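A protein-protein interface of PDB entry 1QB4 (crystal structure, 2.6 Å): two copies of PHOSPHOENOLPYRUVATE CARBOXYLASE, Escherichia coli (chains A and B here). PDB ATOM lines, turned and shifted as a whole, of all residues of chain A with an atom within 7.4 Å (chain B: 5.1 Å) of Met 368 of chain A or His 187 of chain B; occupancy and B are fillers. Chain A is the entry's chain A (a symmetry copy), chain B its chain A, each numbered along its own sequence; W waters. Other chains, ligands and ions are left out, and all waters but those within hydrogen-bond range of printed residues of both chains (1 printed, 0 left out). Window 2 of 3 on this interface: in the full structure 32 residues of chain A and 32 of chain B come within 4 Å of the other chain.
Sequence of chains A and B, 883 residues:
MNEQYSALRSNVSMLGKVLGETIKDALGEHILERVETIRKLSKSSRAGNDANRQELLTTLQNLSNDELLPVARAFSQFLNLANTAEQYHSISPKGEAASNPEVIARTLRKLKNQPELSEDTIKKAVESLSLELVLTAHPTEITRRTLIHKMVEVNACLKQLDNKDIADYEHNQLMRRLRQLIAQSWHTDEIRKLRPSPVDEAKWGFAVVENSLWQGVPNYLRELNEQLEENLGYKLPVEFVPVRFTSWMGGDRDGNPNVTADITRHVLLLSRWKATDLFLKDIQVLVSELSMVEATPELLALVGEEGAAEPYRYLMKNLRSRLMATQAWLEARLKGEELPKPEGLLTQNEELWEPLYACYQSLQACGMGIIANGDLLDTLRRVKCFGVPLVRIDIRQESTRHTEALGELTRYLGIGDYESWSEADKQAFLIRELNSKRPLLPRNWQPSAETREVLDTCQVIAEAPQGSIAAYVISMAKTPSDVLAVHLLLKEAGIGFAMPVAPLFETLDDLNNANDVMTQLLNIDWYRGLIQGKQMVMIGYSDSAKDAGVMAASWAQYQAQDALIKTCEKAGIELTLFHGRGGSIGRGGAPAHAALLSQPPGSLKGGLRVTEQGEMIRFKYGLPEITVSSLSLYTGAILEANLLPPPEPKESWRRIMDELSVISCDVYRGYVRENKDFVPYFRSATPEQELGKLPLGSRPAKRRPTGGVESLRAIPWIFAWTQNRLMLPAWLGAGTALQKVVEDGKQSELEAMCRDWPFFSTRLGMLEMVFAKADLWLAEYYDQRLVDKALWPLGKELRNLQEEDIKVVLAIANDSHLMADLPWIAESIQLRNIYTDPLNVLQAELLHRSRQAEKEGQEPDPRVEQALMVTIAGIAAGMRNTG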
ATOM      1  N   GLU A 289      -3.402  22.013  18.907  1.00  0.00           N
ATOM      2  CA  GLU A 289      -3.960  21.627  17.601  1.00  0.00           C
ATOM      3  C   GLU A 289      -4.354  22.795  16.737  1.00  0.00           C
ATOM      4  O   GLU A 289      -4.475  22.610  15.518  1.00  0.00           O
ATOM      5  CB  GLU A 289      -5.049  20.568  17.739  1.00  0.00           C
ATOM      6  CG  GLU A 289      -4.538  19.148  17.975  1.00  0.00           C
ATOM      7  CD  GLU A 289      -5.624  18.232  18.465  1.00  0.00           C
ATOM      8  OE1 GLU A 289      -6.817  18.641  18.357  1.00  0.00           O
ATOM      9  OE2 GLU A 289      -5.377  17.113  18.954  1.00  0.00           O
ATOM     10  N   SER A 291      -2.984  25.227  14.833  1.00  0.00           N
ATOM     11  CA  SER A 291      -1.818  25.725  14.126  1.00  0.00           C
ATOM     12  C   SER A 291      -2.181  26.312  12.760  1.00  0.00           C
ATOM     13  O   SER A 291      -1.343  26.618  11.942  1.00  0.00           O
ATOM     14  CB  SER A 291      -0.800  24.589  13.839  1.00  0.00           C
ATOM     15  OG  SER A 291      -0.715  23.774  14.984  1.00  0.00           O
ATOM     16  N   MET A 292      -3.444  26.403  12.459  1.00  0.00           N
ATOM     17  CA  MET A 292      -3.982  26.954  11.223  1.00  0.00           C
ATOM     18  C   MET A 292      -3.473  28.383  11.104  1.00  0.00           C
ATOM     19  O   MET A 292      -3.372  29.065  12.136  1.00  0.00           O
ATOM     20  CB  MET A 292      -5.522  26.968  11.403  1.00  0.00           C
ATOM     21  CG  MET A 292      -6.106  25.570  11.364  1.00  0.00           C
ATOM     22  SD  MET A 292      -5.650  24.591  12.808  1.00  0.00           S
ATOM     23  CE  MET A 292      -5.804  22.959  12.099  1.00  0.00           C
ATOM     24  N   VAL A 293      -3.131  28.887   9.936  1.00  0.00           N
ATOM     25  CA  VAL A 293      -2.674  30.274   9.873  1.00  0.00           C
ATOM     26  C   VAL A 293      -3.633  31.060   8.973  1.00  0.00           C
ATOM     27  O   VAL A 293      -3.495  32.263   8.827  1.00  0.00           O
ATOM     28  CB  VAL A 293      -1.282  30.427   9.250  1.00  0.00           C
ATOM     29  CG1 VAL A 293      -0.724  31.788   9.669  1.00  0.00           C
ATOM     30  CG2 VAL A 293      -0.304  29.317   9.581  1.00  0.00           C
ATOM     31  N   GLU A 294      -4.530  30.318   8.332  1.00  0.00           N
ATOM     32  CA  GLU A 294      -5.493  30.952   7.408  1.00  0.00           C
ATOM     33  C   GLU A 294      -6.628  31.484   8.273  1.00  0.00           C
ATOM     34  O   GLU A 294      -7.214  30.703   8.993  1.00  0.00           O
ATOM     35  CB  GLU A 294      -5.902  30.003   6.324  1.00  0.00           C
ATOM     36  N   ALA A 295      -6.841  32.799   8.224  1.00  0.00           N
ATOM     37  CA  ALA A 295      -7.874  33.420   9.053  1.00  0.00           C
ATOM     38  C   ALA A 295      -8.614  34.532   8.329  1.00  0.00           C
ATOM     39  O   ALA A 295      -8.226  34.953   7.242  1.00  0.00           O
ATOM     40  CB  ALA A 295      -7.226  33.900  10.350  1.00  0.00           C
ATOM     41  N   TYR A 312      -5.327  31.595  15.625  1.00  0.00           N
ATOM     42  CA  TYR A 312      -6.171  30.798  16.518  1.00  0.00           C
ATOM     43  C   TYR A 312      -5.428  30.424  17.783  1.00  0.00           C
ATOM     44  O   TYR A 312      -5.933  30.370  18.908  1.00  0.00           O
ATOM     45  CB  TYR A 312      -6.566  29.507  15.812  1.00  0.00           C
ATOM     46  CG  TYR A 312      -7.199  29.767  14.463  1.00  0.00           C
ATOM     47  CD1 TYR A 312      -6.434  29.678  13.309  1.00  0.00           C
ATOM     48  CD2 TYR A 312      -8.536  30.095  14.397  1.00  0.00           C
ATOM     49  CE1 TYR A 312      -7.028  29.914  12.087  1.00  0.00           C
ATOM     50  CE2 TYR A 312      -9.122  30.343  13.169  1.00  0.00           C
ATOM     51  CZ  TYR A 312      -8.359  30.240  12.029  1.00  0.00           C
ATOM     52  OH  TYR A 312      -8.992  30.469  10.836  1.00  0.00           O
ATOM     53  N   CYS A 359     -12.815  31.684  16.822  1.00  0.00           N
ATOM     54  CA  CYS A 359     -12.043  30.685  16.087  1.00  0.00           C
ATOM     55  C   CYS A 359     -12.944  29.813  15.210  1.00  0.00           C
ATOM     56  O   CYS A 359     -12.636  29.672  14.016  1.00  0.00           O
ATOM     57  CB  CYS A 359     -11.176  29.820  16.976  1.00  0.00           C
ATOM     58  SG  CYS A 359      -9.841  30.680  17.834  1.00  0.00           S
ATOM     59  N   TYR A 360     -14.013  29.286  15.787  1.00  0.00           N
ATOM     60  CA  TYR A 360     -14.945  28.457  15.028  1.00  0.00           C
ATOM     61  C   TYR A 360     -15.328  29.103  13.704  1.00  0.00           C
ATOM     62  O   TYR A 360     -15.305  28.464  12.666  1.00  0.00           O
ATOM     63  CB  TYR A 360     -16.213  28.160  15.872  1.00  0.00           C
ATOM     64  CG  TYR A 360     -17.237  27.251  15.229  1.00  0.00           C
ATOM     65  CD1 TYR A 360     -17.393  25.937  15.641  1.00  0.00           C
ATOM     66  CD2 TYR A 360     -18.066  27.686  14.217  1.00  0.00           C
ATOM     67  CE1 TYR A 360     -18.332  25.100  15.068  1.00  0.00           C
ATOM     68  CE2 TYR A 360     -19.005  26.884  13.627  1.00  0.00           C
ATOM     69  CZ  TYR A 360     -19.137  25.578  14.064  1.00  0.00           C
ATOM     70  OH  TYR A 360     -20.084  24.764  13.466  1.00  0.00           O
ATOM     71  N   SER A 362     -13.924  31.604  11.851  1.00  0.00           N
ATOM     72  CA  SER A 362     -12.920  31.689  10.805  1.00  0.00           C
ATOM     73  C   SER A 362     -12.636  30.323  10.196  1.00  0.00           C
ATOM     74  O   SER A 362     -12.564  30.234   8.973  1.00  0.00           O
ATOM     75  CB  SER A 362     -11.565  32.205  11.286  1.00  0.00           C
ATOM     76  OG  SER A 362     -11.702  32.679  12.597  1.00  0.00           O
ATOM     77  N   LEU A 363     -12.427  29.320  11.055  1.00  0.00           N
ATOM     78  CA  LEU A 363     -12.179  27.966  10.564  1.00  0.00           C
ATOM     79  C   LEU A 363     -13.297  27.609   9.603  1.00  0.00           C
ATOM     80  O   LEU A 363     -12.936  27.177   8.494  1.00  0.00           O
ATOM     81  CB  LEU A 363     -11.931  26.995  11.689  1.00  0.00           C
ATOM     82  CG  LEU A 363     -10.714  27.184  12.585  1.00  0.00           C
ATOM     83  CD1 LEU A 363     -10.964  26.716  14.035  1.00  0.00           C
ATOM     84  CD2 LEU A 363      -9.437  26.512  12.119  1.00  0.00           C
ATOM     85  N   GLN A 364     -14.577  27.821   9.858  1.00  0.00           N
ATOM     86  CA  GLN A 364     -15.632  27.505   8.890  1.00  0.00           C
ATOM     87  C   GLN A 364     -15.457  28.324   7.607  1.00  0.00           C
ATOM     88  O   GLN A 364     -15.435  27.810   6.484  1.00  0.00           O
ATOM     89  CB  GLN A 364     -17.014  27.724   9.479  1.00  0.00           C
ATOM     90  CG  GLN A 364     -17.343  26.733  10.583  1.00  0.00           C
ATOM     91  CD  GLN A 364     -18.336  25.706  10.091  1.00  0.00           C
ATOM     92  OE1 GLN A 364     -19.167  26.027   9.239  1.00  0.00           O
ATOM     93  NE2 GLN A 364     -18.294  24.486  10.607  1.00  0.00           N
ATOM     94  N   ALA A 365     -15.302  29.629   7.768  1.00  0.00           N
ATOM     95  CA  ALA A 365     -15.108  30.603   6.718  1.00  0.00           C
ATOM     96  C   ALA A 365     -13.895  30.274   5.834  1.00  0.00           C
ATOM     97  O   ALA A 365     -13.938  30.318   4.600  1.00  0.00           O
ATOM     98  CB  ALA A 365     -14.812  31.959   7.381  1.00  0.00           C
ATOM     99  N   CYS A 366     -12.764  29.944   6.472  1.00  0.00           N
ATOM    100  CA  CYS A 366     -11.528  29.613   5.782  1.00  0.00           C
ATOM    101  C   CYS A 366     -11.425  28.175   5.315  1.00  0.00           C
ATOM    102  O   CYS A 366     -10.290  27.749   5.001  1.00  0.00           O
ATOM    103  CB  CYS A 366     -10.326  29.948   6.687  1.00  0.00           C
ATOM    104  SG  CYS A 366      -9.782  31.701   6.651  1.00  0.00           S
ATOM    105  N   GLY A 367     -12.468  27.361   5.250  1.00  0.00           N
ATOM    106  CA  GLY A 367     -12.395  25.980   4.804  1.00  0.00           C
ATOM    107  C   GLY A 367     -11.989  24.920   5.792  1.00  0.00           C
ATOM    108  O   GLY A 367     -11.754  23.729   5.465  1.00  0.00           O
ATOM    109  N   MET A 368     -11.899  25.222   7.084  1.00  0.00           N
ATOM    110  CA  MET A 368     -11.506  24.207   8.067  1.00  0.00           C
ATOM    111  C   MET A 368     -12.667  23.732   8.918  1.00  0.00           C
ATOM    112  O   MET A 368     -12.544  23.532  10.099  1.00  0.00           O
ATOM    113  CB  MET A 368     -10.330  24.698   8.928  1.00  0.00           C
ATOM    114  CG  MET A 368      -8.966  24.395   8.279  1.00  0.00           C
ATOM    115  SD  MET A 368      -7.735  25.668   8.557  1.00  0.00           S
ATOM    116  CE  MET A 368      -8.334  26.983   7.471  1.00  0.00           C
ATOM    117  N   GLY A 369     -13.776  23.448   8.236  1.00  0.00           N
ATOM    118  CA  GLY A 369     -14.990  23.006   8.893  1.00  0.00           C
ATOM    119  C   GLY A 369     -14.781  21.837   9.815  1.00  0.00           C
ATOM    120  O   GLY A 369     -15.099  21.933  11.009  1.00  0.00           O
ATOM    121  N   ILE A 370     -14.217  20.767   9.255  1.00  0.00           N
ATOM    122  CA  ILE A 370     -13.954  19.550   9.993  1.00  0.00           C
ATOM    123  C   ILE A 370     -13.181  19.766  11.280  1.00  0.00           C
ATOM    124  O   ILE A 370     -13.423  19.001  12.228  1.00  0.00           O
ATOM    125  CB  ILE A 370     -13.205  18.466   9.167  1.00  0.00           C
ATOM    126  CG1 ILE A 370     -13.722  18.432   7.738  1.00  0.00           C
ATOM    127  CG2 ILE A 370     -13.465  17.086   9.737  1.00  0.00           C
ATOM    128  CD1 ILE A 370     -13.027  17.458   6.802  1.00  0.00           C
ATOM    129  N   ILE A 371     -12.274  20.708  11.331  1.00  0.00           N
ATOM    130  CA  ILE A 371     -11.493  20.952  12.542  1.00  0.00           C
ATOM    131  C   ILE A 371     -12.324  21.763  13.553  1.00  0.00           C
ATOM    132  O   ILE A 371     -12.226  21.562  14.753  1.00  0.00           O
ATOM    133  CB  ILE A 371     -10.191  21.746  12.330  1.00  0.00           C
ATOM    134  CG1 ILE A 371      -9.238  21.161  11.253  1.00  0.00           C
ATOM    135  CG2 ILE A 371      -9.444  21.907  13.655  1.00  0.00           C
ATOM    136  CD1 ILE A 371      -8.902  19.701  11.535  1.00  0.00           C
ATOM    137  N   ALA A 372     -13.113  22.686  13.013  1.00  0.00           N
ATOM    138  CA  ALA A 372     -13.978  23.535  13.816  1.00  0.00           C
ATOM    139  C   ALA A 372     -14.984  22.635  14.498  1.00  0.00           C
ATOM    140  O   ALA A 372     -15.011  22.709  15.719  1.00  0.00           O
ATOM    141  CB  ALA A 372     -14.634  24.602  12.968  1.00  0.00           C
ATOM    142  N   ASN A 373     -15.648  21.741  13.770  1.00  0.00           N
ATOM    143  CA  ASN A 373     -16.641  20.878  14.333  1.00  0.00           C
ATOM    144  C   ASN A 373     -16.183  19.722  15.180  1.00  0.00           C
ATOM    145  O   ASN A 373     -17.008  18.811  15.433  1.00  0.00           O
ATOM    146  CB  ASN A 373     -17.559  20.252  13.231  1.00  0.00           C
ATOM    147  CG  ASN A 373     -18.608  21.294  12.844  1.00  0.00           C
ATOM    148  OD1 ASN A 373     -19.472  21.623  13.669  1.00  0.00           O
ATOM    149  ND2 ASN A 373     -18.500  21.785  11.628  1.00  0.00           N
ATOM    150  N   GLY A 374     -14.950  19.731  15.609  1.00  0.00           N
ATOM    151  CA  GLY A 374     -14.340  18.698  16.392  1.00  0.00           C
ATOM    152  C   GLY A 374     -14.183  19.157  17.817  1.00  0.00           C
ATOM    153  O   GLY A 374     -15.207  19.533  18.370  1.00  0.00           O
ATOM    154  N   THR B  22     -10.862  14.621   2.537  1.00  0.00           N
ATOM    155  CA  THR B  22     -10.326  15.788   3.204  1.00  0.00           C
ATOM    156  C   THR B  22      -9.690  16.800   2.275  1.00  0.00           C
ATOM    157  O   THR B  22      -9.797  17.984   2.522  1.00  0.00           O
ATOM    158  CB  THR B  22      -9.266  15.350   4.242  1.00  0.00           C
ATOM    159  OG1 THR B  22      -9.804  14.562   5.305  1.00  0.00           O
ATOM    160  CG2 THR B  22      -8.550  16.555   4.830  1.00  0.00           C
ATOM    161  N   ALA B  26     -10.871  20.563   1.662  1.00  0.00           N
ATOM    162  CA  ALA B  26      -9.840  21.522   1.864  1.00  0.00           C
ATOM    163  C   ALA B  26      -9.741  22.723   0.949  1.00  0.00           C
ATOM    164  O   ALA B  26     -10.141  23.846   1.240  1.00  0.00           O
ATOM    165  CB  ALA B  26      -8.475  20.811   1.942  1.00  0.00           C
ATOM    166  N   LEU B  27      -9.104  22.517  -0.185  1.00  0.00           N
ATOM    167  CA  LEU B  27      -8.810  23.546  -1.157  1.00  0.00           C
ATOM    168  C   LEU B  27      -8.987  23.094  -2.580  1.00  0.00           C
ATOM    169  O   LEU B  27      -9.151  23.917  -3.497  1.00  0.00           O
ATOM    170  CB  LEU B  27      -7.352  24.008  -0.917  1.00  0.00           C
ATOM    171  CG  LEU B  27      -6.283  22.937  -0.709  1.00  0.00           C
ATOM    172  CD1 LEU B  27      -4.974  23.402  -1.344  1.00  0.00           C
ATOM    173  CD2 LEU B  27      -6.045  22.644   0.775  1.00  0.00           C
ATOM    174  N   ARG B  73       3.078  17.619  -0.207  1.00  0.00           N
ATOM    175  CA  ARG B  73       2.452  17.163   1.037  1.00  0.00           C
ATOM    176  C   ARG B  73       1.452  16.066   0.751  1.00  0.00           C
ATOM    177  O   ARG B  73       1.336  15.077   1.479  1.00  0.00           O
ATOM    178  CB  ARG B  73       1.861  18.326   1.823  1.00  0.00           C
ATOM    179  CG  ARG B  73       2.823  19.393   2.320  1.00  0.00           C
ATOM    180  CD  ARG B  73       2.178  20.375   3.320  1.00  0.00           C
ATOM    181  NE  ARG B  73       1.683  19.661   4.520  1.00  0.00           N
ATOM    182  CZ  ARG B  73       0.437  19.659   4.926  1.00  0.00           C
ATOM    183  NH1 ARG B  73      -0.477  20.348   4.220  1.00  0.00           N
ATOM    184  NH2 ARG B  73       0.052  18.977   5.998  1.00  0.00           N
ATOM    185  N   ALA B 183      -7.871  15.056   8.916  1.00  0.00           N
ATOM    186  CA  ALA B 183      -7.972  16.469   8.596  1.00  0.00           C
ATOM    187  C   ALA B 183      -6.891  17.242   9.364  1.00  0.00           C
ATOM    188  O   ALA B 183      -6.169  18.057   8.812  1.00  0.00           O
ATOM    189  CB  ALA B 183      -9.351  17.017   8.903  1.00  0.00           C
ATOM    190  N   GLN B 184      -6.788  17.036  10.665  1.00  0.00           N
ATOM    191  CA  GLN B 184      -5.765  17.687  11.469  1.00  0.00           C
ATOM    192  C   GLN B 184      -4.439  17.652  10.696  1.00  0.00           C
ATOM    193  O   GLN B 184      -3.926  18.729  10.434  1.00  0.00           O
ATOM    194  CB  GLN B 184      -5.506  17.026  12.816  1.00  0.00           C
ATOM    195  CG  GLN B 184      -6.216  17.480  14.035  1.00  0.00           C
ATOM    196  CD  GLN B 184      -6.745  16.453  15.010  1.00  0.00           C
ATOM    197  OE1 GLN B 184      -6.070  15.899  15.906  1.00  0.00           O
ATOM    198  NE2 GLN B 184      -8.035  16.143  14.888  1.00  0.00           N
ATOM    199  N   SER B 185      -3.910  16.482  10.347  1.00  0.00           N
ATOM    200  CA  SER B 185      -2.675  16.348   9.617  1.00  0.00           C
ATOM    201  C   SER B 185      -2.597  17.099   8.299  1.00  0.00           C
ATOM    202  O   SER B 185      -1.501  17.582   8.006  1.00  0.00           O
ATOM    203  CB  SER B 185      -2.384  14.886   9.270  1.00  0.00           C
ATOM    204  OG  SER B 185      -2.045  14.120  10.409  1.00  0.00           O
ATOM    205  N   TRP B 186      -3.688  17.181   7.533  1.00  0.00           N
ATOM    206  CA  TRP B 186      -3.619  17.899   6.263  1.00  0.00           C
ATOM    207  C   TRP B 186      -3.537  19.391   6.508  1.00  0.00           C
ATOM    208  O   TRP B 186      -2.791  20.096   5.838  1.00  0.00           O
ATOM    209  CB  TRP B 186      -4.776  17.506   5.370  1.00  0.00           C
ATOM    210  CG  TRP B 186      -4.780  18.368   4.146  1.00  0.00           C
ATOM    211  CD1 TRP B 186      -5.701  19.302   3.806  1.00  0.00           C
ATOM    212  CD2 TRP B 186      -3.799  18.362   3.115  1.00  0.00           C
ATOM    213  NE1 TRP B 186      -5.351  19.865   2.610  1.00  0.00           N
ATOM    214  CE2 TRP B 186      -4.187  19.308   2.158  1.00  0.00           C
ATOM    215  CE3 TRP B 186      -2.632  17.621   2.892  1.00  0.00           C
ATOM    216  CZ2 TRP B 186      -3.462  19.574   1.005  1.00  0.00           C
ATOM    217  CZ3 TRP B 186      -1.899  17.883   1.765  1.00  0.00           C
ATOM    218  CH2 TRP B 186      -2.306  18.848   0.843  1.00  0.00           C
ATOM    219  N   HIS B 187      -4.198  19.879   7.554  1.00  0.00           N
ATOM    220  CA  HIS B 187      -4.231  21.297   7.869  1.00  0.00           C
ATOM    221  C   HIS B 187      -3.239  21.695   8.923  1.00  0.00           C
ATOM    222  O   HIS B 187      -2.794  22.855   8.958  1.00  0.00           O
ATOM    223  CB  HIS B 187      -5.628  21.749   8.386  1.00  0.00           C
ATOM    224  CG  HIS B 187      -6.661  21.714   7.304  1.00  0.00           C
ATOM    225  ND1 HIS B 187      -6.551  22.502   6.194  1.00  0.00           N
ATOM    226  CD2 HIS B 187      -7.786  21.008   7.157  1.00  0.00           C
ATOM    227  CE1 HIS B 187      -7.564  22.310   5.405  1.00  0.00           C
ATOM    228  NE2 HIS B 187      -8.352  21.384   5.969  1.00  0.00           N
ATOM    229  N   THR B 188      -2.885  20.768   9.800  1.00  0.00           N
ATOM    230  CA  THR B 188      -1.912  21.163  10.835  1.00  0.00           C
ATOM    231  C   THR B 188      -0.530  21.209  10.222  1.00  0.00           C
ATOM    232  O   THR B 188       0.222  20.261  10.497  1.00  0.00           O
ATOM    233  CB  THR B 188      -1.826  20.208  12.030  1.00  0.00           C
ATOM    234  OG1 THR B 188      -3.148  19.935  12.533  1.00  0.00           O
ATOM    235  CG2 THR B 188      -1.028  20.906  13.147  1.00  0.00           C
ATOM    236  N   ASP B 189      -0.216  22.202   9.404  1.00  0.00           N
ATOM    237  CA  ASP B 189       1.139  22.181   8.853  1.00  0.00           C
ATOM    238  C   ASP B 189       2.027  23.129   9.689  1.00  0.00           C
ATOM    239  O   ASP B 189       1.753  24.260  10.107  1.00  0.00           O
ATOM    240  CB  ASP B 189       1.230  22.443   7.382  1.00  0.00           C
ATOM    241  CG  ASP B 189       1.145  23.907   6.977  1.00  0.00           C
ATOM    242  OD1 ASP B 189       2.017  24.328   6.171  1.00  0.00           O
ATOM    243  OD2 ASP B 189       0.211  24.596   7.469  1.00  0.00           O
HETATM  244  O   HOH W   1      -4.718  20.025  14.450  1.00  0.00           O
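OE2 of Glu 289 of chain A sits close to OE1 of Gln 184 of chain B, 3.4 Å away.
The backbone carbonyl oxygen of Gln 184 of chain B is in hydrogen-bond range of the side-chain hydroxyl of Thr 188 of chain B (2.5 Å).
O of Leu 363 of chain A sits at hydrogen-bond distance from N of Met 368 of chain A.
Thr 188 of chain B touches Ser 291 of chain A.
CE of Met 292 of chain A touches CB of His 187 of chain B, at 3.9 Å.
His 187 of chain B touches Met 368 of chain A.
Ile 371 of chain A touches Ala 183 of chain B (CD1 to CB, 3.8 Å).
Gln 184 of chain B touches Ile 371 of chain A (N to CD1, 3.5 Å).
Of the printed residues of chain B, Glu 289 of chain A touches Gln 184.
Of the printed residues of chain B, Ser 291 of chain A touches Thr 188 (3.4 Å).
Printed residues of chain B within 4 Å of Met 368 of chain A: His 187 (3.7 Å).
Of the printed residues of chain A, Ala 183 of chain B touches Ile 371.
Of the printed residues of chain A, Gln 184 of chain B touches Glu 289 (3.4 Å) and Ile 371 (3.5 Å).
Of the printed residues of chain A, Thr 188 of chain B touches Ser 291 (3.4 Å).
The nearest printed residue of chain B that does not touch Met 368 of chain A is Ala 26 of chain B (6.3 Å).
The nearest printed residue of chain B that does not touch Ser 291 of chain A is Asp 189 of chain B (4.3 Å).
Of the 11 printed residues of chain B, 4 touch a printed residue of chain A.
Hydrophobic or aromatic side chains of chain A that line the printed part of chain B: Met 292, Met 368 and Ile 371.
Among the printed residues, 6 pairs touch across the chains.
Among the printed residues, no Asp or Glu carboxylate lies within 4 Å of a Lys or Arg side-chain nitrogen of the other chain.
No position is printed for both chains.
Of the 6 pairs that touch across the chains among the printed residues, none has its exchanged pair printed and touching as well.
Water W1 lies within hydrogen-bond range of the side-chain hydroxyl (OG1) of Thr 188 of chain B (2.5 Å) and the backbone carbonyl oxygen (O) of Glu 289 of chain A (2.8 Å).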
